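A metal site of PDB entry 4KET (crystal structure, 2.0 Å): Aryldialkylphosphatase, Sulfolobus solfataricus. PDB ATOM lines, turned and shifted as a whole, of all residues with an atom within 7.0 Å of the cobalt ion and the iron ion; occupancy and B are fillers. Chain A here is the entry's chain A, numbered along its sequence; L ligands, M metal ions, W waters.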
ATOM      1  N   HIS A  22     -17.935  -3.935 -30.921  1.00  0.00           N
ATOM      2  CA  HIS A  22     -16.814  -3.606 -30.033  1.00  0.00           C
ATOM      3  C   HIS A  22     -17.082  -4.115 -28.635  1.00  0.00           C
ATOM      4  O   HIS A  22     -17.693  -3.409 -27.812  1.00  0.00           O
ATOM      5  CB  HIS A  22     -16.570  -2.094 -30.017  1.00  0.00           C
ATOM      6  CG  HIS A  22     -15.291  -1.670 -29.306  1.00  0.00           C
ATOM      7  ND1 HIS A  22     -14.468  -0.721 -29.792  1.00  0.00           N
ATOM      8  CD2 HIS A  22     -14.712  -2.114 -28.101  1.00  0.00           C
ATOM      9  CE1 HIS A  22     -13.405  -0.556 -28.954  1.00  0.00           C
ATOM     10  NE2 HIS A  22     -13.565  -1.404 -27.921  1.00  0.00           N
ATOM     11  N   GLU A  23     -16.667  -5.349 -28.371  1.00  0.00           N
ATOM     12  CA  GLU A  23     -16.766  -5.944 -27.025  1.00  0.00           C
ATOM     13  C   GLU A  23     -15.489  -6.714 -26.712  1.00  0.00           C
ATOM     14  O   GLU A  23     -14.835  -7.241 -27.624  1.00  0.00           O
ATOM     15  CB  GLU A  23     -17.960  -6.907 -26.937  1.00  0.00           C
ATOM     16  CG  GLU A  23     -19.278  -6.358 -27.446  1.00  0.00           C
ATOM     17  CD  GLU A  23     -19.854  -5.264 -26.569  1.00  0.00           C
ATOM     18  OE1 GLU A  23     -20.711  -4.494 -27.069  1.00  0.00           O
ATOM     19  OE2 GLU A  23     -19.451  -5.164 -25.383  1.00  0.00           O
ATOM     20  N   HIS A  24     -15.138  -6.806 -25.436  1.00  0.00           N
ATOM     21  CA  HIS A  24     -13.913  -7.512 -25.042  1.00  0.00           C
ATOM     22  C   HIS A  24     -14.222  -8.700 -24.182  1.00  0.00           C
ATOM     23  O   HIS A  24     -14.876  -8.585 -23.141  1.00  0.00           O
ATOM     24  CB  HIS A  24     -12.983  -6.564 -24.274  1.00  0.00           C
ATOM     25  CG  HIS A  24     -12.528  -5.349 -25.057  1.00  0.00           C
ATOM     26  ND1 HIS A  24     -11.441  -5.382 -25.858  1.00  0.00           N
ATOM     27  CD2 HIS A  24     -13.012  -4.040 -25.096  1.00  0.00           C
ATOM     28  CE1 HIS A  24     -11.249  -4.146 -26.390  1.00  0.00           C
ATOM     29  NE2 HIS A  24     -12.220  -3.342 -25.933  1.00  0.00           N
ATOM     30  N   VAL A  27      -9.567  -8.362 -20.956  1.00  0.00           N
ATOM     31  CA  VAL A  27      -8.504  -7.371 -21.132  1.00  0.00           C
ATOM     32  C   VAL A  27      -7.515  -7.471 -19.968  1.00  0.00           C
ATOM     33  O   VAL A  27      -7.918  -7.620 -18.812  1.00  0.00           O
ATOM     34  CB  VAL A  27      -9.089  -5.945 -21.224  1.00  0.00           C
ATOM     35  CG1 VAL A  27      -7.981  -4.902 -21.100  1.00  0.00           C
ATOM     36  CG2 VAL A  27      -9.844  -5.755 -22.536  1.00  0.00           C
ATOM     37  N   PRO A  67     -11.931  -6.223 -30.308  1.00  0.00           N
ATOM     38  CA  PRO A  67     -10.724  -5.473 -30.680  1.00  0.00           C
ATOM     39  C   PRO A  67      -9.651  -5.470 -29.600  1.00  0.00           C
ATOM     40  O   PRO A  67      -8.923  -4.488 -29.444  1.00  0.00           O
ATOM     41  CB  PRO A  67     -11.259  -4.063 -30.921  1.00  0.00           C
ATOM     42  CG  PRO A  67     -12.432  -3.952 -29.991  1.00  0.00           C
ATOM     43  CD  PRO A  67     -13.001  -5.338 -29.795  1.00  0.00           C
ATOM     44  N   THR A  68      -9.548  -6.571 -28.857  1.00  0.00           N
ATOM     45  CA  THR A  68      -8.448  -6.763 -27.918  1.00  0.00           C
ATOM     46  C   THR A  68      -7.216  -7.101 -28.750  1.00  0.00           C
ATOM     47  O   THR A  68      -7.190  -8.145 -29.421  1.00  0.00           O
ATOM     48  CB  THR A  68      -8.728  -7.950 -26.968  1.00  0.00           C
ATOM     49  OG1 THR A  68      -9.991  -7.775 -26.332  1.00  0.00           O
ATOM     50  CG2 THR A  68      -7.629  -8.057 -25.910  1.00  0.00           C
ATOM     51  N   LEU A  72      -3.630  -4.817 -24.877  1.00  0.00           N
ATOM     52  CA  LEU A  72      -4.862  -5.169 -24.144  1.00  0.00           C
ATOM     53  C   LEU A  72      -4.925  -6.648 -23.788  1.00  0.00           C
ATOM     54  O   LEU A  72      -5.939  -7.114 -23.253  1.00  0.00           O
ATOM     55  CB  LEU A  72      -6.101  -4.792 -24.954  1.00  0.00           C
ATOM     56  CG  LEU A  72      -6.266  -3.301 -25.267  1.00  0.00           C
ATOM     57  CD1 LEU A  72      -7.434  -3.073 -26.227  1.00  0.00           C
ATOM     58  CD2 LEU A  72      -6.460  -2.502 -23.989  1.00  0.00           C
ATOM     59  N   TYR A  97      -2.344  -1.141 -29.433  1.00  0.00           N
ATOM     60  CA  TYR A  97      -3.082  -0.190 -28.609  1.00  0.00           C
ATOM     61  C   TYR A  97      -2.082   0.534 -27.703  1.00  0.00           C
ATOM     62  O   TYR A  97      -1.602  -0.037 -26.715  1.00  0.00           O
ATOM     63  CB  TYR A  97      -4.118  -0.964 -27.783  1.00  0.00           C
ATOM     64  CG  TYR A  97      -5.051  -0.144 -26.918  1.00  0.00           C
ATOM     65  CD1 TYR A  97      -4.654   0.326 -25.675  1.00  0.00           C
ATOM     66  CD2 TYR A  97      -6.361   0.115 -27.330  1.00  0.00           C
ATOM     67  CE1 TYR A  97      -5.517   1.056 -24.879  1.00  0.00           C
ATOM     68  CE2 TYR A  97      -7.222   0.850 -26.543  1.00  0.00           C
ATOM     69  CZ  TYR A  97      -6.802   1.315 -25.309  1.00  0.00           C
ATOM     70  OH  TYR A  97      -7.664   2.037 -24.517  1.00  0.00           O
ATOM     71  N   TYR A  99      -1.065   4.750 -26.077  1.00  0.00           N
ATOM     72  CA  TYR A  99      -1.467   6.161 -25.919  1.00  0.00           C
ATOM     73  C   TYR A  99      -0.308   7.127 -26.108  1.00  0.00           C
ATOM     74  O   TYR A  99      -0.508   8.291 -26.440  1.00  0.00           O
ATOM     75  CB  TYR A  99      -2.067   6.421 -24.533  1.00  0.00           C
ATOM     76  CG  TYR A  99      -3.393   5.779 -24.225  1.00  0.00           C
ATOM     77  CD1 TYR A  99      -4.119   5.079 -25.188  1.00  0.00           C
ATOM     78  CD2 TYR A  99      -3.960   5.914 -22.961  1.00  0.00           C
ATOM     79  CE1 TYR A  99      -5.341   4.501 -24.887  1.00  0.00           C
ATOM     80  CE2 TYR A  99      -5.173   5.359 -22.656  1.00  0.00           C
ATOM     81  CZ  TYR A  99      -5.870   4.659 -23.612  1.00  0.00           C
ATOM     82  OH  TYR A  99      -7.085   4.111 -23.257  1.00  0.00           O
ATOM     83  N   KCX A 137      -6.799  -2.711 -35.268  1.00  0.00           N
ATOM     84  CA  KCX A 137      -7.242  -1.810 -34.184  1.00  0.00           C
ATOM     85  CB  KCX A 137      -7.644  -2.650 -32.974  1.00  0.00           C
ATOM     86  CG  KCX A 137      -7.761  -1.842 -31.671  1.00  0.00           C
ATOM     87  CD  KCX A 137      -9.005  -0.955 -31.638  1.00  0.00           C
ATOM     88  CE  KCX A 137      -9.083  -0.170 -30.325  1.00  0.00           C
ATOM     89  NZ  KCX A 137      -9.613  -0.972 -29.220  1.00  0.00           N
ATOM     90  C   KCX A 137      -6.105  -0.884 -33.813  1.00  0.00           C
ATOM     91  O   KCX A 137      -4.980  -1.336 -33.558  1.00  0.00           O
ATOM     92  CX  KCX A 137     -10.311  -0.486 -28.179  1.00  0.00           C
ATOM     93  OQ1 KCX A 137     -10.710  -1.412 -27.300  1.00  0.00           O
ATOM     94  OQ2 KCX A 137     -10.598   0.715 -27.981  1.00  0.00           O
ATOM     95  N   ILE A 138      -6.386   0.414 -33.794  1.00  0.00           N
ATOM     96  CA  ILE A 138      -5.420   1.420 -33.362  1.00  0.00           C
ATOM     97  C   ILE A 138      -6.061   2.332 -32.311  1.00  0.00           C
ATOM     98  O   ILE A 138      -7.291   2.355 -32.153  1.00  0.00           O
ATOM     99  CB  ILE A 138      -4.921   2.261 -34.547  1.00  0.00           C
ATOM    100  CG1 ILE A 138      -6.087   3.040 -35.169  1.00  0.00           C
ATOM    101  CG2 ILE A 138      -4.244   1.367 -35.579  1.00  0.00           C
ATOM    102  CD1 ILE A 138      -5.737   3.775 -36.452  1.00  0.00           C
ATOM    103  N   ALA A 139      -5.226   3.107 -31.608  1.00  0.00           N
ATOM    104  CA  ALA A 139      -5.719   3.957 -30.530  1.00  0.00           C
ATOM    105  C   ALA A 139      -5.034   5.309 -30.456  1.00  0.00           C
ATOM    106  O   ALA A 139      -3.911   5.492 -30.925  1.00  0.00           O
ATOM    107  CB  ALA A 139      -5.597   3.228 -29.192  1.00  0.00           C
ATOM    108  N   ASP A 141      -5.458   8.705 -27.320  1.00  0.00           N
ATOM    109  CA  ASP A 141      -6.286   9.173 -26.216  1.00  0.00           C
ATOM    110  C   ASP A 141      -5.860  10.569 -25.783  1.00  0.00           C
ATOM    111  O   ASP A 141      -5.489  11.395 -26.632  1.00  0.00           O
ATOM    112  CB  ASP A 141      -6.238   8.154 -25.063  1.00  0.00           C
ATOM    113  CG  ASP A 141      -7.489   8.204 -24.188  1.00  0.00           C
ATOM    114  OD1 ASP A 141      -7.589   9.082 -23.312  1.00  0.00           O
ATOM    115  OD2 ASP A 141      -8.388   7.345 -24.366  1.00  0.00           O
ATOM    116  N   THR A 169     -10.919   2.111 -34.484  1.00  0.00           N
ATOM    117  CA  THR A 169     -10.079   2.939 -33.644  1.00  0.00           C
ATOM    118  C   THR A 169     -10.658   3.146 -32.259  1.00  0.00           C
ATOM    119  O   THR A 169     -11.862   3.046 -32.035  1.00  0.00           O
ATOM    120  CB  THR A 169      -9.788   4.327 -34.240  1.00  0.00           C
ATOM    121  OG1 THR A 169     -10.854   5.237 -33.901  1.00  0.00           O
ATOM    122  CG2 THR A 169      -9.625   4.245 -35.778  1.00  0.00           C
ATOM    123  N   HIS A 170      -9.756   3.407 -31.325  1.00  0.00           N
ATOM    124  CA  HIS A 170     -10.046   3.939 -30.023  1.00  0.00           C
ATOM    125  C   HIS A 170      -9.641   5.390 -30.106  1.00  0.00           C
ATOM    126  O   HIS A 170      -8.524   5.701 -30.515  1.00  0.00           O
ATOM    127  CB  HIS A 170      -9.188   3.194 -29.013  1.00  0.00           C
ATOM    128  CG  HIS A 170      -9.239   3.771 -27.600  1.00  0.00           C
ATOM    129  ND1 HIS A 170      -9.900   3.149 -26.591  1.00  0.00           N
ATOM    130  CD2 HIS A 170      -8.661   4.919 -27.069  1.00  0.00           C
ATOM    131  CE1 HIS A 170      -9.752   3.887 -25.472  1.00  0.00           C
ATOM    132  NE2 HIS A 170      -8.992   4.963 -25.761  1.00  0.00           N
ATOM    133  N   SER A 171     -10.537   6.288 -29.741  1.00  0.00           N
ATOM    134  CA  SER A 171     -10.178   7.696 -29.649  1.00  0.00           C
ATOM    135  C   SER A 171     -10.732   8.328 -28.369  1.00  0.00           C
ATOM    136  O   SER A 171     -11.523   7.719 -27.657  1.00  0.00           O
ATOM    137  CB  SER A 171     -10.658   8.478 -30.883  1.00  0.00           C
ATOM    138  OG  SER A 171     -12.009   8.880 -30.741  1.00  0.00           O
ATOM    139  N   GLY A 198     -13.777   5.289 -32.993  1.00  0.00           N
ATOM    140  CA  GLY A 198     -14.389   4.758 -31.778  1.00  0.00           C
ATOM    141  C   GLY A 198     -14.578   5.779 -30.679  1.00  0.00           C
ATOM    142  O   GLY A 198     -13.911   6.818 -30.647  1.00  0.00           O
ATOM    143  N   HIS A 199     -15.521   5.466 -29.790  1.00  0.00           N
ATOM    144  CA  HIS A 199     -15.720   6.180 -28.526  1.00  0.00           C
ATOM    145  C   HIS A 199     -16.284   7.582 -28.697  1.00  0.00           C
ATOM    146  O   HIS A 199     -16.206   8.422 -27.786  1.00  0.00           O
ATOM    147  CB  HIS A 199     -14.429   6.160 -27.688  1.00  0.00           C
ATOM    148  CG  HIS A 199     -13.843   4.765 -27.483  1.00  0.00           C
ATOM    149  ND1 HIS A 199     -14.610   3.649 -27.526  1.00  0.00           N
ATOM    150  CD2 HIS A 199     -12.536   4.330 -27.254  1.00  0.00           C
ATOM    151  CE1 HIS A 199     -13.829   2.557 -27.323  1.00  0.00           C
ATOM    152  NE2 HIS A 199     -12.564   2.970 -27.152  1.00  0.00           N
ATOM    153  N   ASP A 222     -20.219   3.518 -28.721  1.00  0.00           N
ATOM    154  CA  ASP A 222     -19.793   2.149 -28.460  1.00  0.00           C
ATOM    155  C   ASP A 222     -19.424   1.841 -27.009  1.00  0.00           C
ATOM    156  O   ASP A 222     -18.816   0.802 -26.737  1.00  0.00           O
ATOM    157  CB  ASP A 222     -18.617   1.824 -29.394  1.00  0.00           C
ATOM    158  CG  ASP A 222     -17.475   2.832 -29.281  1.00  0.00           C
ATOM    159  OD1 ASP A 222     -16.652   2.917 -30.224  1.00  0.00           O
ATOM    160  OD2 ASP A 222     -17.377   3.528 -28.246  1.00  0.00           O
ATOM    161  N   ARG A 223     -19.783   2.726 -26.089  1.00  0.00           N
ATOM    162  CA  ARG A 223     -19.447   2.513 -24.674  1.00  0.00           C
ATOM    163  C   ARG A 223     -20.657   2.615 -23.759  1.00  0.00           C
ATOM    164  O   ARG A 223     -20.563   3.074 -22.623  1.00  0.00           O
ATOM    165  CB  ARG A 223     -18.351   3.471 -24.224  1.00  0.00           C
ATOM    166  CG  ARG A 223     -16.955   3.025 -24.615  1.00  0.00           C
ATOM    167  CD  ARG A 223     -15.924   4.080 -24.233  1.00  0.00           C
ATOM    168  NE  ARG A 223     -14.589   3.489 -24.027  1.00  0.00           N
ATOM    169  CZ  ARG A 223     -13.483   4.194 -23.848  1.00  0.00           C
ATOM    170  NH1 ARG A 223     -13.528   5.524 -23.868  1.00  0.00           N
ATOM    171  NH2 ARG A 223     -12.329   3.566 -23.662  1.00  0.00           N
ATOM    172  N   ASP A 256     -18.374  -1.850 -25.435  1.00  0.00           N
ATOM    173  CA  ASP A 256     -16.967  -1.958 -25.041  1.00  0.00           C
ATOM    174  C   ASP A 256     -16.931  -2.685 -23.689  1.00  0.00           C
ATOM    175  O   ASP A 256     -16.100  -2.399 -22.841  1.00  0.00           O
ATOM    176  CB  ASP A 256     -16.332  -0.564 -24.933  1.00  0.00           C
ATOM    177  CG  ASP A 256     -14.785  -0.572 -24.883  1.00  0.00           C
ATOM    178  OD1 ASP A 256     -14.058  -1.477 -25.389  1.00  0.00           O
ATOM    179  OD2 ASP A 256     -14.287   0.454 -24.358  1.00  0.00           O
ATOM    180  N   TYR A 257     -17.842  -3.624 -23.503  1.00  0.00           N
ATOM    181  CA  TYR A 257     -17.872  -4.384 -22.257  1.00  0.00           C
ATOM    182  C   TYR A 257     -16.660  -5.307 -22.166  1.00  0.00           C
ATOM    183  O   TYR A 257     -16.287  -5.953 -23.146  1.00  0.00           O
ATOM    184  CB  TYR A 257     -19.159  -5.194 -22.094  1.00  0.00           C
ATOM    185  CG  TYR A 257     -19.264  -5.826 -20.724  1.00  0.00           C
ATOM    186  CD1 TYR A 257     -19.155  -7.204 -20.550  1.00  0.00           C
ATOM    187  CD2 TYR A 257     -19.416  -5.029 -19.601  1.00  0.00           C
ATOM    188  CE1 TYR A 257     -19.233  -7.764 -19.285  1.00  0.00           C
ATOM    189  CE2 TYR A 257     -19.493  -5.575 -18.340  1.00  0.00           C
ATOM    190  CZ  TYR A 257     -19.390  -6.944 -18.186  1.00  0.00           C
ATOM    191  OH  TYR A 257     -19.468  -7.482 -16.920  1.00  0.00           O
ATOM    192  N   CYS A 258     -16.047  -5.333 -20.986  1.00  0.00           N
ATOM    193  CA  CYS A 258     -14.970  -6.258 -20.694  1.00  0.00           C
ATOM    194  C   CYS A 258     -15.456  -7.319 -19.714  1.00  0.00           C
ATOM    195  O   CYS A 258     -15.683  -7.023 -18.530  1.00  0.00           O
ATOM    196  CB  CYS A 258     -13.775  -5.509 -20.102  1.00  0.00           C
ATOM    197  SG  CYS A 258     -13.158  -4.208 -21.196  1.00  0.00           S
HETATM  198  C1  LIG L   1     -10.094  -0.803 -22.572  1.00  0.00           C
HETATM  199  O1  LIG L   1     -10.903  -1.290 -23.659  1.00  0.00           O
HETATM  200  C2  LIG L   1      -9.672   0.621 -22.879  1.00  0.00           C
HETATM  201  O2  LIG L   1     -10.258   1.022 -24.133  1.00  0.00           O
HETATM  202 CO    CO M   1     -11.189   1.724 -26.649  1.00  0.00          CO
HETATM  203 FE    FE M   2     -12.432  -1.442 -26.319  1.00  0.00          FE
HETATM  204  O   HOH W   1     -12.168   0.195 -25.826  1.00  0.00           O
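O of Ile 138 sits at hydrogen-bond distance from N of His 170, at 2.8 Å. O of Asp 222 is in hydrogen-bond range of N of Asp 256, at 3.0 Å. The backbone NH of His 199 sits at hydrogen-bond distance from the side-chain carboxylate of Asp 222 (2.8 Å). A ring nitrogen (NE2) of His 170 is in hydrogen-bond range of the side-chain carboxylate (OD2) of Asp 141 (2.8 Å). O of Tyr 257 is in hydrogen-bond range of N of His 24 (2.7 Å). OH of Tyr 97 sits close to NE2 of His 170, 3.4 Å away. NE2 of His 170 lies within hydrogen-bond range of OH of Tyr 99, 3.3 Å away. The side-chain hydroxyl (OG1) of Thr 68 is in hydrogen-bond range of a ring nitrogen (ND1) of His 24 (2.8 Å).
The cobalt ion is bound by OQ2 of KCX 137 (1.8 Å). The cobalt ion is bound by ND1 of His 170 (1.9 Å). A ring nitrogen (NE2) of His 199 is bound to the cobalt ion (1.9 Å). The cobalt ion is bound by water W1 (2.0 Å). The cobalt ion has four donor atoms within binding distance. Slightly farther from the cobalt ion lies an oxygen (O2) of the ligand (2.8 Å).
Within 4 Å of the iron ion: His 22, His 24, KCX 137 and Asp 256. The nearest printed residue that does not touch the iron ion is His 199 (4.4 Å).
Arg 223 touches the cobalt ion (NH2 to CO, 3.7 Å). Along chain A the residues within 4 Å of the cobalt ion span positions 22 to 223. The nearest printed residue that does not touch the cobalt ion is Asp 256 (4.1 Å).
The iron ion is bound by water W1 (1.7 Å), the side-chain carboxylate (OD1) of Asp 256 (1.9 Å), a ring nitrogen (NE2) of His 24 (2.0 Å), a ring nitrogen (NE2) of His 22 (2.0 Å) and OQ1 of KCX 137 (2.0 Å).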
